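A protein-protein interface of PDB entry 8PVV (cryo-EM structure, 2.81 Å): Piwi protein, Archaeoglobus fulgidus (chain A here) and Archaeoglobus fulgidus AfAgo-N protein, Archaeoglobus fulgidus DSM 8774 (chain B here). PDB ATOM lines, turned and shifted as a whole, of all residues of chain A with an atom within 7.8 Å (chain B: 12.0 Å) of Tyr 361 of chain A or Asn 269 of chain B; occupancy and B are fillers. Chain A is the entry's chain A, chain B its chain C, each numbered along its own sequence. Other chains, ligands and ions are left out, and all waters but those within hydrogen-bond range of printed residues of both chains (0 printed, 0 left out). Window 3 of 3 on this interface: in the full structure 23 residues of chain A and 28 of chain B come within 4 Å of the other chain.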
ATOM      1  N   GLU A   3      15.933  19.406 -11.359  1.00  0.00           N
ATOM      2  CA  GLU A   3      16.375  20.472 -12.240  1.00  0.00           C
ATOM      3  C   GLU A   3      15.327  20.731 -13.315  1.00  0.00           C
ATOM      4  O   GLU A   3      14.443  19.908 -13.564  1.00  0.00           O
ATOM      5  CB  GLU A   3      17.721  20.128 -12.887  1.00  0.00           C
ATOM      6  CG  GLU A   3      17.671  18.962 -13.855  1.00  0.00           C
ATOM      7  CD  GLU A   3      18.368  17.729 -13.316  1.00  0.00           C
ATOM      8  OE1 GLU A   3      18.143  17.384 -12.137  1.00  0.00           O
ATOM      9  OE2 GLU A   3      19.143  17.106 -14.070  1.00  0.00           O
ATOM     10  N   TYR A   4      15.427  21.900 -13.945  1.00  0.00           N
ATOM     11  CA  TYR A   4      14.520  22.261 -15.022  1.00  0.00           C
ATOM     12  C   TYR A   4      15.255  23.108 -16.050  1.00  0.00           C
ATOM     13  O   TYR A   4      16.267  23.746 -15.755  1.00  0.00           O
ATOM     14  CB  TYR A   4      13.276  23.001 -14.498  1.00  0.00           C
ATOM     15  CG  TYR A   4      13.467  24.476 -14.210  1.00  0.00           C
ATOM     16  CD1 TYR A   4      13.251  25.434 -15.194  1.00  0.00           C
ATOM     17  CD2 TYR A   4      13.841  24.913 -12.948  1.00  0.00           C
ATOM     18  CE1 TYR A   4      13.420  26.777 -14.932  1.00  0.00           C
ATOM     19  CE2 TYR A   4      14.008  26.255 -12.678  1.00  0.00           C
ATOM     20  CZ  TYR A   4      13.797  27.181 -13.672  1.00  0.00           C
ATOM     21  OH  TYR A   4      13.963  28.520 -13.404  1.00  0.00           O
ATOM     22  N   LYS A   5      14.725  23.097 -17.271  1.00  0.00           N
ATOM     23  CA  LYS A   5      15.258  23.884 -18.373  1.00  0.00           C
ATOM     24  C   LYS A   5      14.100  24.431 -19.193  1.00  0.00           C
ATOM     25  O   LYS A   5      13.096  23.742 -19.398  1.00  0.00           O
ATOM     26  CB  LYS A   5      16.189  23.050 -19.260  1.00  0.00           C
ATOM     27  CG  LYS A   5      17.061  23.874 -20.187  1.00  0.00           C
ATOM     28  CD  LYS A   5      17.960  22.985 -21.025  1.00  0.00           C
ATOM     29  CE  LYS A   5      19.023  23.795 -21.748  1.00  0.00           C
ATOM     30  NZ  LYS A   5      18.531  25.146 -22.133  1.00  0.00           N
ATOM     31  N   LYS A 315      10.524  22.906 -18.711  1.00  0.00           N
ATOM     32  CA  LYS A 315      10.606  21.450 -18.674  1.00  0.00           C
ATOM     33  C   LYS A 315      11.219  21.044 -17.339  1.00  0.00           C
ATOM     34  O   LYS A 315      12.404  21.291 -17.098  1.00  0.00           O
ATOM     35  CB  LYS A 315      11.432  20.927 -19.846  1.00  0.00           C
ATOM     36  CG  LYS A 315      11.179  21.670 -21.147  1.00  0.00           C
ATOM     37  CD  LYS A 315      12.060  21.160 -22.270  1.00  0.00           C
ATOM     38  CE  LYS A 315      13.432  21.799 -22.241  1.00  0.00           C
ATOM     39  NZ  LYS A 315      13.457  23.068 -23.016  1.00  0.00           N
ATOM     40  N   LYS A 317      12.405  18.225 -14.749  1.00  0.00           N
ATOM     41  CA  LYS A 317      12.915  16.857 -14.816  1.00  0.00           C
ATOM     42  C   LYS A 317      12.460  16.091 -13.583  1.00  0.00           C
ATOM     43  O   LYS A 317      13.106  16.113 -12.535  1.00  0.00           O
ATOM     44  CB  LYS A 317      14.432  16.862 -14.933  1.00  0.00           C
ATOM     45  CG  LYS A 317      15.022  15.557 -15.428  1.00  0.00           C
ATOM     46  CD  LYS A 317      16.505  15.699 -15.713  1.00  0.00           C
ATOM     47  CE  LYS A 317      17.117  14.368 -16.109  1.00  0.00           C
ATOM     48  NZ  LYS A 317      16.619  13.263 -15.252  1.00  0.00           N
ATOM     49  N   TYR A 323       8.955  13.808 -17.574  1.00  0.00           N
ATOM     50  CA  TYR A 323       9.171  15.244 -17.535  1.00  0.00           C
ATOM     51  C   TYR A 323       7.846  15.962 -17.342  1.00  0.00           C
ATOM     52  O   TYR A 323       6.796  15.490 -17.782  1.00  0.00           O
ATOM     53  CB  TYR A 323       9.839  15.748 -18.822  1.00  0.00           C
ATOM     54  CG  TYR A 323      11.277  15.320 -18.979  1.00  0.00           C
ATOM     55  CD1 TYR A 323      12.314  16.206 -18.728  1.00  0.00           C
ATOM     56  CD2 TYR A 323      11.599  14.032 -19.376  1.00  0.00           C
ATOM     57  CE1 TYR A 323      13.629  15.821 -18.868  1.00  0.00           C
ATOM     58  CE2 TYR A 323      12.908  13.637 -19.515  1.00  0.00           C
ATOM     59  CZ  TYR A 323      13.920  14.535 -19.261  1.00  0.00           C
ATOM     60  OH  TYR A 323      15.232  14.146 -19.402  1.00  0.00           O
ATOM     61  N   TRP A 355      17.261   5.506 -28.380  1.00  0.00           N
ATOM     62  CA  TRP A 355      18.405   6.392 -28.242  1.00  0.00           C
ATOM     63  C   TRP A 355      19.508   5.741 -27.423  1.00  0.00           C
ATOM     64  O   TRP A 355      19.248   5.010 -26.464  1.00  0.00           O
ATOM     65  CB  TRP A 355      17.992   7.703 -27.577  1.00  0.00           C
ATOM     66  CG  TRP A 355      16.764   8.332 -28.136  1.00  0.00           C
ATOM     67  CD1 TRP A 355      16.273   8.202 -29.401  1.00  0.00           C
ATOM     68  CD2 TRP A 355      15.862   9.196 -27.442  1.00  0.00           C
ATOM     69  NE1 TRP A 355      15.122   8.936 -29.538  1.00  0.00           N
ATOM     70  CE2 TRP A 355      14.848   9.556 -28.348  1.00  0.00           C
ATOM     71  CE3 TRP A 355      15.815   9.702 -26.141  1.00  0.00           C
ATOM     72  CZ2 TRP A 355      13.799  10.398 -27.995  1.00  0.00           C
ATOM     73  CZ3 TRP A 355      14.774  10.536 -25.793  1.00  0.00           C
ATOM     74  CH2 TRP A 355      13.780  10.875 -26.714  1.00  0.00           C
ATOM     75  N   THR A 356      20.748   6.010 -27.813  1.00  0.00           N
ATOM     76  CA  THR A 356      21.887   5.669 -26.983  1.00  0.00           C
ATOM     77  C   THR A 356      22.024   6.679 -25.848  1.00  0.00           C
ATOM     78  O   THR A 356      21.454   7.774 -25.883  1.00  0.00           O
ATOM     79  CB  THR A 356      23.170   5.624 -27.813  1.00  0.00           C
ATOM     80  OG1 THR A 356      24.257   5.174 -26.994  1.00  0.00           O
ATOM     81  CG2 THR A 356      23.492   7.000 -28.374  1.00  0.00           C
ATOM     82  N   SER A 357      22.788   6.295 -24.824  1.00  0.00           N
ATOM     83  CA  SER A 357      22.939   7.157 -23.655  1.00  0.00           C
ATOM     84  C   SER A 357      23.637   8.467 -23.999  1.00  0.00           C
ATOM     85  O   SER A 357      23.402   9.485 -23.339  1.00  0.00           O
ATOM     86  CB  SER A 357      23.705   6.422 -22.556  1.00  0.00           C
ATOM     87  OG  SER A 357      24.875   5.813 -23.070  1.00  0.00           O
ATOM     88  N   GLU A 358      24.494   8.465 -25.020  1.00  0.00           N
ATOM     89  CA  GLU A 358      25.236   9.675 -25.363  1.00  0.00           C
ATOM     90  C   GLU A 358      24.318  10.759 -25.918  1.00  0.00           C
ATOM     91  O   GLU A 358      24.511  11.948 -25.634  1.00  0.00           O
ATOM     92  CB  GLU A 358      26.342   9.345 -26.364  1.00  0.00           C
ATOM     93  CG  GLU A 358      27.443  10.390 -26.437  1.00  0.00           C
ATOM     94  CD  GLU A 358      27.156  11.469 -27.462  1.00  0.00           C
ATOM     95  OE1 GLU A 358      26.846  11.123 -28.621  1.00  0.00           O
ATOM     96  OE2 GLU A 358      27.234  12.663 -27.105  1.00  0.00           O
ATOM     97  N   GLU A 359      23.322  10.374 -26.711  1.00  0.00           N
ATOM     98  CA  GLU A 359      22.432  11.317 -27.376  1.00  0.00           C
ATOM     99  C   GLU A 359      21.139  11.575 -26.612  1.00  0.00           C
ATOM    100  O   GLU A 359      20.275  12.301 -27.122  1.00  0.00           O
ATOM    101  CB  GLU A 359      22.090  10.808 -28.778  1.00  0.00           C
ATOM    102  CG  GLU A 359      21.027   9.722 -28.777  1.00  0.00           C
ATOM    103  CD  GLU A 359      20.780   9.137 -30.149  1.00  0.00           C
ATOM    104  OE1 GLU A 359      21.653   9.283 -31.030  1.00  0.00           O
ATOM    105  OE2 GLU A 359      19.708   8.532 -30.345  1.00  0.00           O
ATOM    106  N   TYR A 360      20.984  10.989 -25.422  1.00  0.00           N
ATOM    107  CA  TYR A 360      19.708  11.042 -24.715  1.00  0.00           C
ATOM    108  C   TYR A 360      19.290  12.468 -24.394  1.00  0.00           C
ATOM    109  O   TYR A 360      18.134  12.846 -24.611  1.00  0.00           O
ATOM    110  CB  TYR A 360      19.780  10.220 -23.431  1.00  0.00           C
ATOM    111  CG  TYR A 360      18.418   9.838 -22.914  1.00  0.00           C
ATOM    112  CD1 TYR A 360      17.763   8.710 -23.379  1.00  0.00           C
ATOM    113  CD2 TYR A 360      17.778  10.626 -21.970  1.00  0.00           C
ATOM    114  CE1 TYR A 360      16.514   8.375 -22.907  1.00  0.00           C
ATOM    115  CE2 TYR A 360      16.533  10.299 -21.493  1.00  0.00           C
ATOM    116  CZ  TYR A 360      15.904   9.172 -21.964  1.00  0.00           C
ATOM    117  OH  TYR A 360      14.660   8.843 -21.492  1.00  0.00           O
ATOM    118  N   TYR A 361      20.207  13.266 -23.842  1.00  0.00           N
ATOM    119  CA  TYR A 361      19.860  14.626 -23.443  1.00  0.00           C
ATOM    120  C   TYR A 361      19.350  15.426 -24.632  1.00  0.00           C
ATOM    121  O   TYR A 361      18.273  16.037 -24.576  1.00  0.00           O
ATOM    122  CB  TYR A 361      21.079  15.303 -22.814  1.00  0.00           C
ATOM    123  CG  TYR A 361      20.806  16.670 -22.230  1.00  0.00           C
ATOM    124  CD1 TYR A 361      21.017  17.821 -22.978  1.00  0.00           C
ATOM    125  CD2 TYR A 361      20.343  16.810 -20.931  1.00  0.00           C
ATOM    126  CE1 TYR A 361      20.772  19.072 -22.448  1.00  0.00           C
ATOM    127  CE2 TYR A 361      20.095  18.058 -20.392  1.00  0.00           C
ATOM    128  CZ  TYR A 361      20.310  19.184 -21.155  1.00  0.00           C
ATOM    129  OH  TYR A 361      20.063  20.427 -20.620  1.00  0.00           O
ATOM    130  N   HIS A 362      20.102  15.404 -25.732  1.00  0.00           N
ATOM    131  CA  HIS A 362      19.711  16.166 -26.909  1.00  0.00           C
ATOM    132  C   HIS A 362      18.382  15.674 -27.466  1.00  0.00           C
ATOM    133  O   HIS A 362      17.506  16.477 -27.790  1.00  0.00           O
ATOM    134  CB  HIS A 362      20.805  16.087 -27.972  1.00  0.00           C
ATOM    135  CG  HIS A 362      20.676  17.121 -29.045  1.00  0.00           C
ATOM    136  ND1 HIS A 362      20.975  18.451 -28.836  1.00  0.00           N
ATOM    137  CD2 HIS A 362      20.271  17.025 -30.333  1.00  0.00           C
ATOM    138  CE1 HIS A 362      20.764  19.127 -29.951  1.00  0.00           C
ATOM    139  NE2 HIS A 362      20.336  18.286 -30.874  1.00  0.00           N
ATOM    140  N   ASN A 363      18.206  14.353 -27.567  1.00  0.00           N
ATOM    141  CA  ASN A 363      16.983  13.830 -28.172  1.00  0.00           C
ATOM    142  C   ASN A 363      15.756  14.139 -27.323  1.00  0.00           C
ATOM    143  O   ASN A 363      14.706  14.533 -27.856  1.00  0.00           O
ATOM    144  CB  ASN A 363      17.115  12.327 -28.402  1.00  0.00           C
ATOM    145  CG  ASN A 363      17.996  11.997 -29.585  1.00  0.00           C
ATOM    146  OD1 ASN A 363      18.910  12.748 -29.922  1.00  0.00           O
ATOM    147  ND2 ASN A 363      17.723  10.868 -30.228  1.00  0.00           N
ATOM    148  N   VAL A 364      15.859  13.969 -26.002  1.00  0.00           N
ATOM    149  CA  VAL A 364      14.710  14.248 -25.148  1.00  0.00           C
ATOM    150  C   VAL A 364      14.387  15.734 -25.164  1.00  0.00           C
ATOM    151  O   VAL A 364      13.215  16.126 -25.200  1.00  0.00           O
ATOM    152  CB  VAL A 364      14.933  13.726 -23.715  1.00  0.00           C
ATOM    153  CG1 VAL A 364      16.069  14.451 -23.026  1.00  0.00           C
ATOM    154  CG2 VAL A 364      13.666  13.895 -22.908  1.00  0.00           C
ATOM    155  N   HIS A 365      15.409  16.590 -25.164  1.00  0.00           N
ATOM    156  CA  HIS A 365      15.099  18.008 -25.221  1.00  0.00           C
ATOM    157  C   HIS A 365      14.495  18.381 -26.565  1.00  0.00           C
ATOM    158  O   HIS A 365      13.593  19.218 -26.616  1.00  0.00           O
ATOM    159  CB  HIS A 365      16.344  18.830 -24.912  1.00  0.00           C
ATOM    160  CG  HIS A 365      16.495  19.142 -23.456  1.00  0.00           C
ATOM    161  ND1 HIS A 365      16.596  18.159 -22.496  1.00  0.00           N
ATOM    162  CD2 HIS A 365      16.546  20.321 -22.795  1.00  0.00           C
ATOM    163  CE1 HIS A 365      16.708  18.720 -21.306  1.00  0.00           C
ATOM    164  NE2 HIS A 365      16.680  20.031 -21.459  1.00  0.00           N
ATOM    165  N   GLU A 366      14.925  17.732 -27.648  1.00  0.00           N
ATOM    166  CA  GLU A 366      14.323  17.994 -28.951  1.00  0.00           C
ATOM    167  C   GLU A 366      12.843  17.642 -28.950  1.00  0.00           C
ATOM    168  O   GLU A 366      12.007  18.425 -29.418  1.00  0.00           O
ATOM    169  CB  GLU A 366      15.052  17.211 -30.043  1.00  0.00           C
ATOM    170  CG  GLU A 366      16.447  17.710 -30.355  1.00  0.00           C
ATOM    171  CD  GLU A 366      16.447  18.914 -31.263  1.00  0.00           C
ATOM    172  OE1 GLU A 366      15.956  19.981 -30.836  1.00  0.00           O
ATOM    173  OE2 GLU A 366      16.937  18.792 -32.404  1.00  0.00           O
ATOM    174  N   ILE A 367      12.495  16.467 -28.420  1.00  0.00           N
ATOM    175  CA  ILE A 367      11.085  16.091 -28.434  1.00  0.00           C
ATOM    176  C   ILE A 367      10.275  16.989 -27.502  1.00  0.00           C
ATOM    177  O   ILE A 367       9.111  17.295 -27.786  1.00  0.00           O
ATOM    178  CB  ILE A 367      10.892  14.599 -28.100  1.00  0.00           C
ATOM    179  CG1 ILE A 367      11.389  14.274 -26.696  1.00  0.00           C
ATOM    180  CG2 ILE A 367      11.604  13.735 -29.127  1.00  0.00           C
ATOM    181  CD1 ILE A 367      11.017  12.893 -26.232  1.00  0.00           C
ATOM    182  N   LEU A 368      10.865  17.449 -26.395  1.00  0.00           N
ATOM    183  CA  LEU A 368      10.128  18.350 -25.510  1.00  0.00           C
ATOM    184  C   LEU A 368       9.900  19.717 -26.154  1.00  0.00           C
ATOM    185  O   LEU A 368       8.790  20.265 -26.078  1.00  0.00           O
ATOM    186  CB  LEU A 368      10.857  18.493 -24.178  1.00  0.00           C
ATOM    187  CG  LEU A 368      10.983  17.214 -23.351  1.00  0.00           C
ATOM    188  CD1 LEU A 368      11.791  17.474 -22.098  1.00  0.00           C
ATOM    189  CD2 LEU A 368       9.610  16.670 -23.006  1.00  0.00           C
ATOM    190  N   ASP A 369      10.926  20.286 -26.796  1.00  0.00           N
ATOM    191  CA  ASP A 369      10.710  21.539 -27.512  1.00  0.00           C
ATOM    192  C   ASP A 369       9.693  21.366 -28.629  1.00  0.00           C
ATOM    193  O   ASP A 369       8.888  22.266 -28.878  1.00  0.00           O
ATOM    194  CB  ASP A 369      12.008  22.129 -28.078  1.00  0.00           C
ATOM    195  CG  ASP A 369      13.076  22.367 -27.025  1.00  0.00           C
ATOM    196  OD1 ASP A 369      14.054  21.605 -26.953  1.00  0.00           O
ATOM    197  OD2 ASP A 369      12.938  23.340 -26.258  1.00  0.00           O
ATOM    198  N   GLN B 162      16.313   9.315  -8.978  1.00  0.00           N
ATOM    199  CA  GLN B 162      17.765   9.263  -8.820  1.00  0.00           C
ATOM    200  C   GLN B 162      18.218   8.071  -7.979  1.00  0.00           C
ATOM    201  O   GLN B 162      19.319   8.087  -7.419  1.00  0.00           O
ATOM    202  CB  GLN B 162      18.312  10.571  -8.234  1.00  0.00           C
ATOM    203  CG  GLN B 162      18.161  11.763  -9.166  1.00  0.00           C
ATOM    204  CD  GLN B 162      18.688  13.049  -8.565  1.00  0.00           C
ATOM    205  OE1 GLN B 162      19.116  13.081  -7.411  1.00  0.00           O
ATOM    206  NE2 GLN B 162      18.665  14.120  -9.349  1.00  0.00           N
ATOM    207  N   VAL B 265      15.654  23.633  -9.597  1.00  0.00           N
ATOM    208  CA  VAL B 265      16.744  24.528  -9.963  1.00  0.00           C
ATOM    209  C   VAL B 265      16.874  24.566 -11.479  1.00  0.00           C
ATOM    210  O   VAL B 265      16.606  23.577 -12.168  1.00  0.00           O
ATOM    211  CB  VAL B 265      18.064  24.078  -9.299  1.00  0.00           C
ATOM    212  CG1 VAL B 265      19.195  25.051  -9.605  1.00  0.00           C
ATOM    213  CG2 VAL B 265      17.873  23.925  -7.802  1.00  0.00           C
ATOM    214  N   GLU B 266      17.276  25.722 -12.003  1.00  0.00           N
ATOM    215  CA  GLU B 266      17.486  25.886 -13.435  1.00  0.00           C
ATOM    216  C   GLU B 266      18.890  25.424 -13.798  1.00  0.00           C
ATOM    217  O   GLU B 266      19.876  25.929 -13.250  1.00  0.00           O
ATOM    218  CB  GLU B 266      17.274  27.338 -13.856  1.00  0.00           C
ATOM    219  CG  GLU B 266      17.120  27.524 -15.359  1.00  0.00           C
ATOM    220  CD  GLU B 266      16.308  28.752 -15.716  1.00  0.00           C
ATOM    221  OE1 GLU B 266      15.834  29.443 -14.790  1.00  0.00           O
ATOM    222  OE2 GLU B 266      16.141  29.027 -16.923  1.00  0.00           O
ATOM    223  N   VAL B 267      18.979  24.471 -14.721  1.00  0.00           N
ATOM    224  CA  VAL B 267      20.250  23.945 -15.202  1.00  0.00           C
ATOM    225  C   VAL B 267      20.447  24.404 -16.639  1.00  0.00           C
ATOM    226  O   VAL B 267      19.507  24.393 -17.443  1.00  0.00           O
ATOM    227  CB  VAL B 267      20.310  22.408 -15.085  1.00  0.00           C
ATOM    228  CG1 VAL B 267      19.202  21.753 -15.901  1.00  0.00           C
ATOM    229  CG2 VAL B 267      21.678  21.895 -15.513  1.00  0.00           C
ATOM    230  N   SER B 268      21.666  24.831 -16.956  1.00  0.00           N
ATOM    231  CA  SER B 268      21.997  25.379 -18.265  1.00  0.00           C
ATOM    232  C   SER B 268      22.927  24.416 -18.988  1.00  0.00           C
ATOM    233  O   SER B 268      23.957  24.009 -18.439  1.00  0.00           O
ATOM    234  CB  SER B 268      22.648  26.756 -18.131  1.00  0.00           C
ATOM    235  OG  SER B 268      22.980  27.286 -19.402  1.00  0.00           O
ATOM    236  N   ASN B 269      22.562  24.056 -20.215  1.00  0.00           N
ATOM    237  CA  ASN B 269      23.385  23.185 -21.043  1.00  0.00           C
ATOM    238  C   ASN B 269      23.163  23.479 -22.524  1.00  0.00           C
ATOM    239  O   ASN B 269      22.681  24.552 -22.887  1.00  0.00           O
ATOM    240  CB  ASN B 269      23.086  21.715 -20.748  1.00  0.00           C
ATOM    241  CG  ASN B 269      23.940  21.160 -19.628  1.00  0.00           C
ATOM    242  OD1 ASN B 269      25.151  21.377 -19.591  1.00  0.00           O
ATOM    243  ND2 ASN B 269      23.315  20.436 -18.708  1.00  0.00           N
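OH of Tyr 4 of chain A is in hydrogen-bond range of OE1 of Glu 266 of chain B (2.5 Å).
The backbone carbonyl oxygen (O) of Tyr 4 of chain A lies within hydrogen-bond range of the backbone NH (N) of Val 267 of chain B, 3.0 Å away.
N of Tyr 4 of chain A lies within hydrogen-bond range of O of Val 265 of chain B, at 2.7 Å.
O of Lys 5 of chain A sits at hydrogen-bond distance from N of Lys 315 of chain A, 2.8 Å away.
ND1 of His 365 of chain A lies close to O of Tyr 361 of chain A (3.4 Å).
O of Glu 3 of chain A is in hydrogen-bond range of N of Lys 317 of chain A (2.9 Å).
Val 265 of chain B touches Glu 3 of chain A (O to CA, 3.1 Å).
Glu 3 of chain A touches Val 267 of chain B (CB to CG1, 3.7 Å).
Lys 5 of chain A touches Val 267 of chain B.
CE of Lys 5 of chain A touches N of Asn 269 of chain B, 3.9 Å away.
Tyr 361 of chain A touches Asn 269 of chain B (OH to CB, 3.3 Å).
Of the printed residues of chain B, Tyr 4 of chain A touches Val 265 (2.7 Å), Glu 266 (2.5 Å) and Val 267 (3.0 Å).
Lys 5 of chain A touches two residues of chain B.
Glu 358 of chain A touches none of the printed residues of chain B.
No residue of chain B comes within 4 Å of Tyr 360 of chain A.
Tyr 361 of chain A touches one residue of chain B.
No residue of chain B comes within 4 Å of Asn 363 of chain A.
No residue of chain B comes within 4 Å of Val 364 of chain A.
Printed residues of chain A within 4 Å of Val 267 of chain B: Glu 3, Tyr 4 and Lys 5.
No residue of chain A comes within 4 Å of Ser 268 of chain B.
Of chain A, only Lys 5 (3.9 Å) and Tyr 361 (3.3 Å) come within 4 Å of Asn 269 of chain B.
The nearest residue of chain A that does not touch Asn 269 of chain B is His 365 of chain A (6.7 Å).
Printed residues of chain B that touch a printed residue of chain A: Val 265, Glu 266, Val 267 and Asn 269.
Along chain B the printed residues that touch a printed residue of chain A span positions 265 to 269.
Among the printed residues, 8 pairs touch across the chains.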
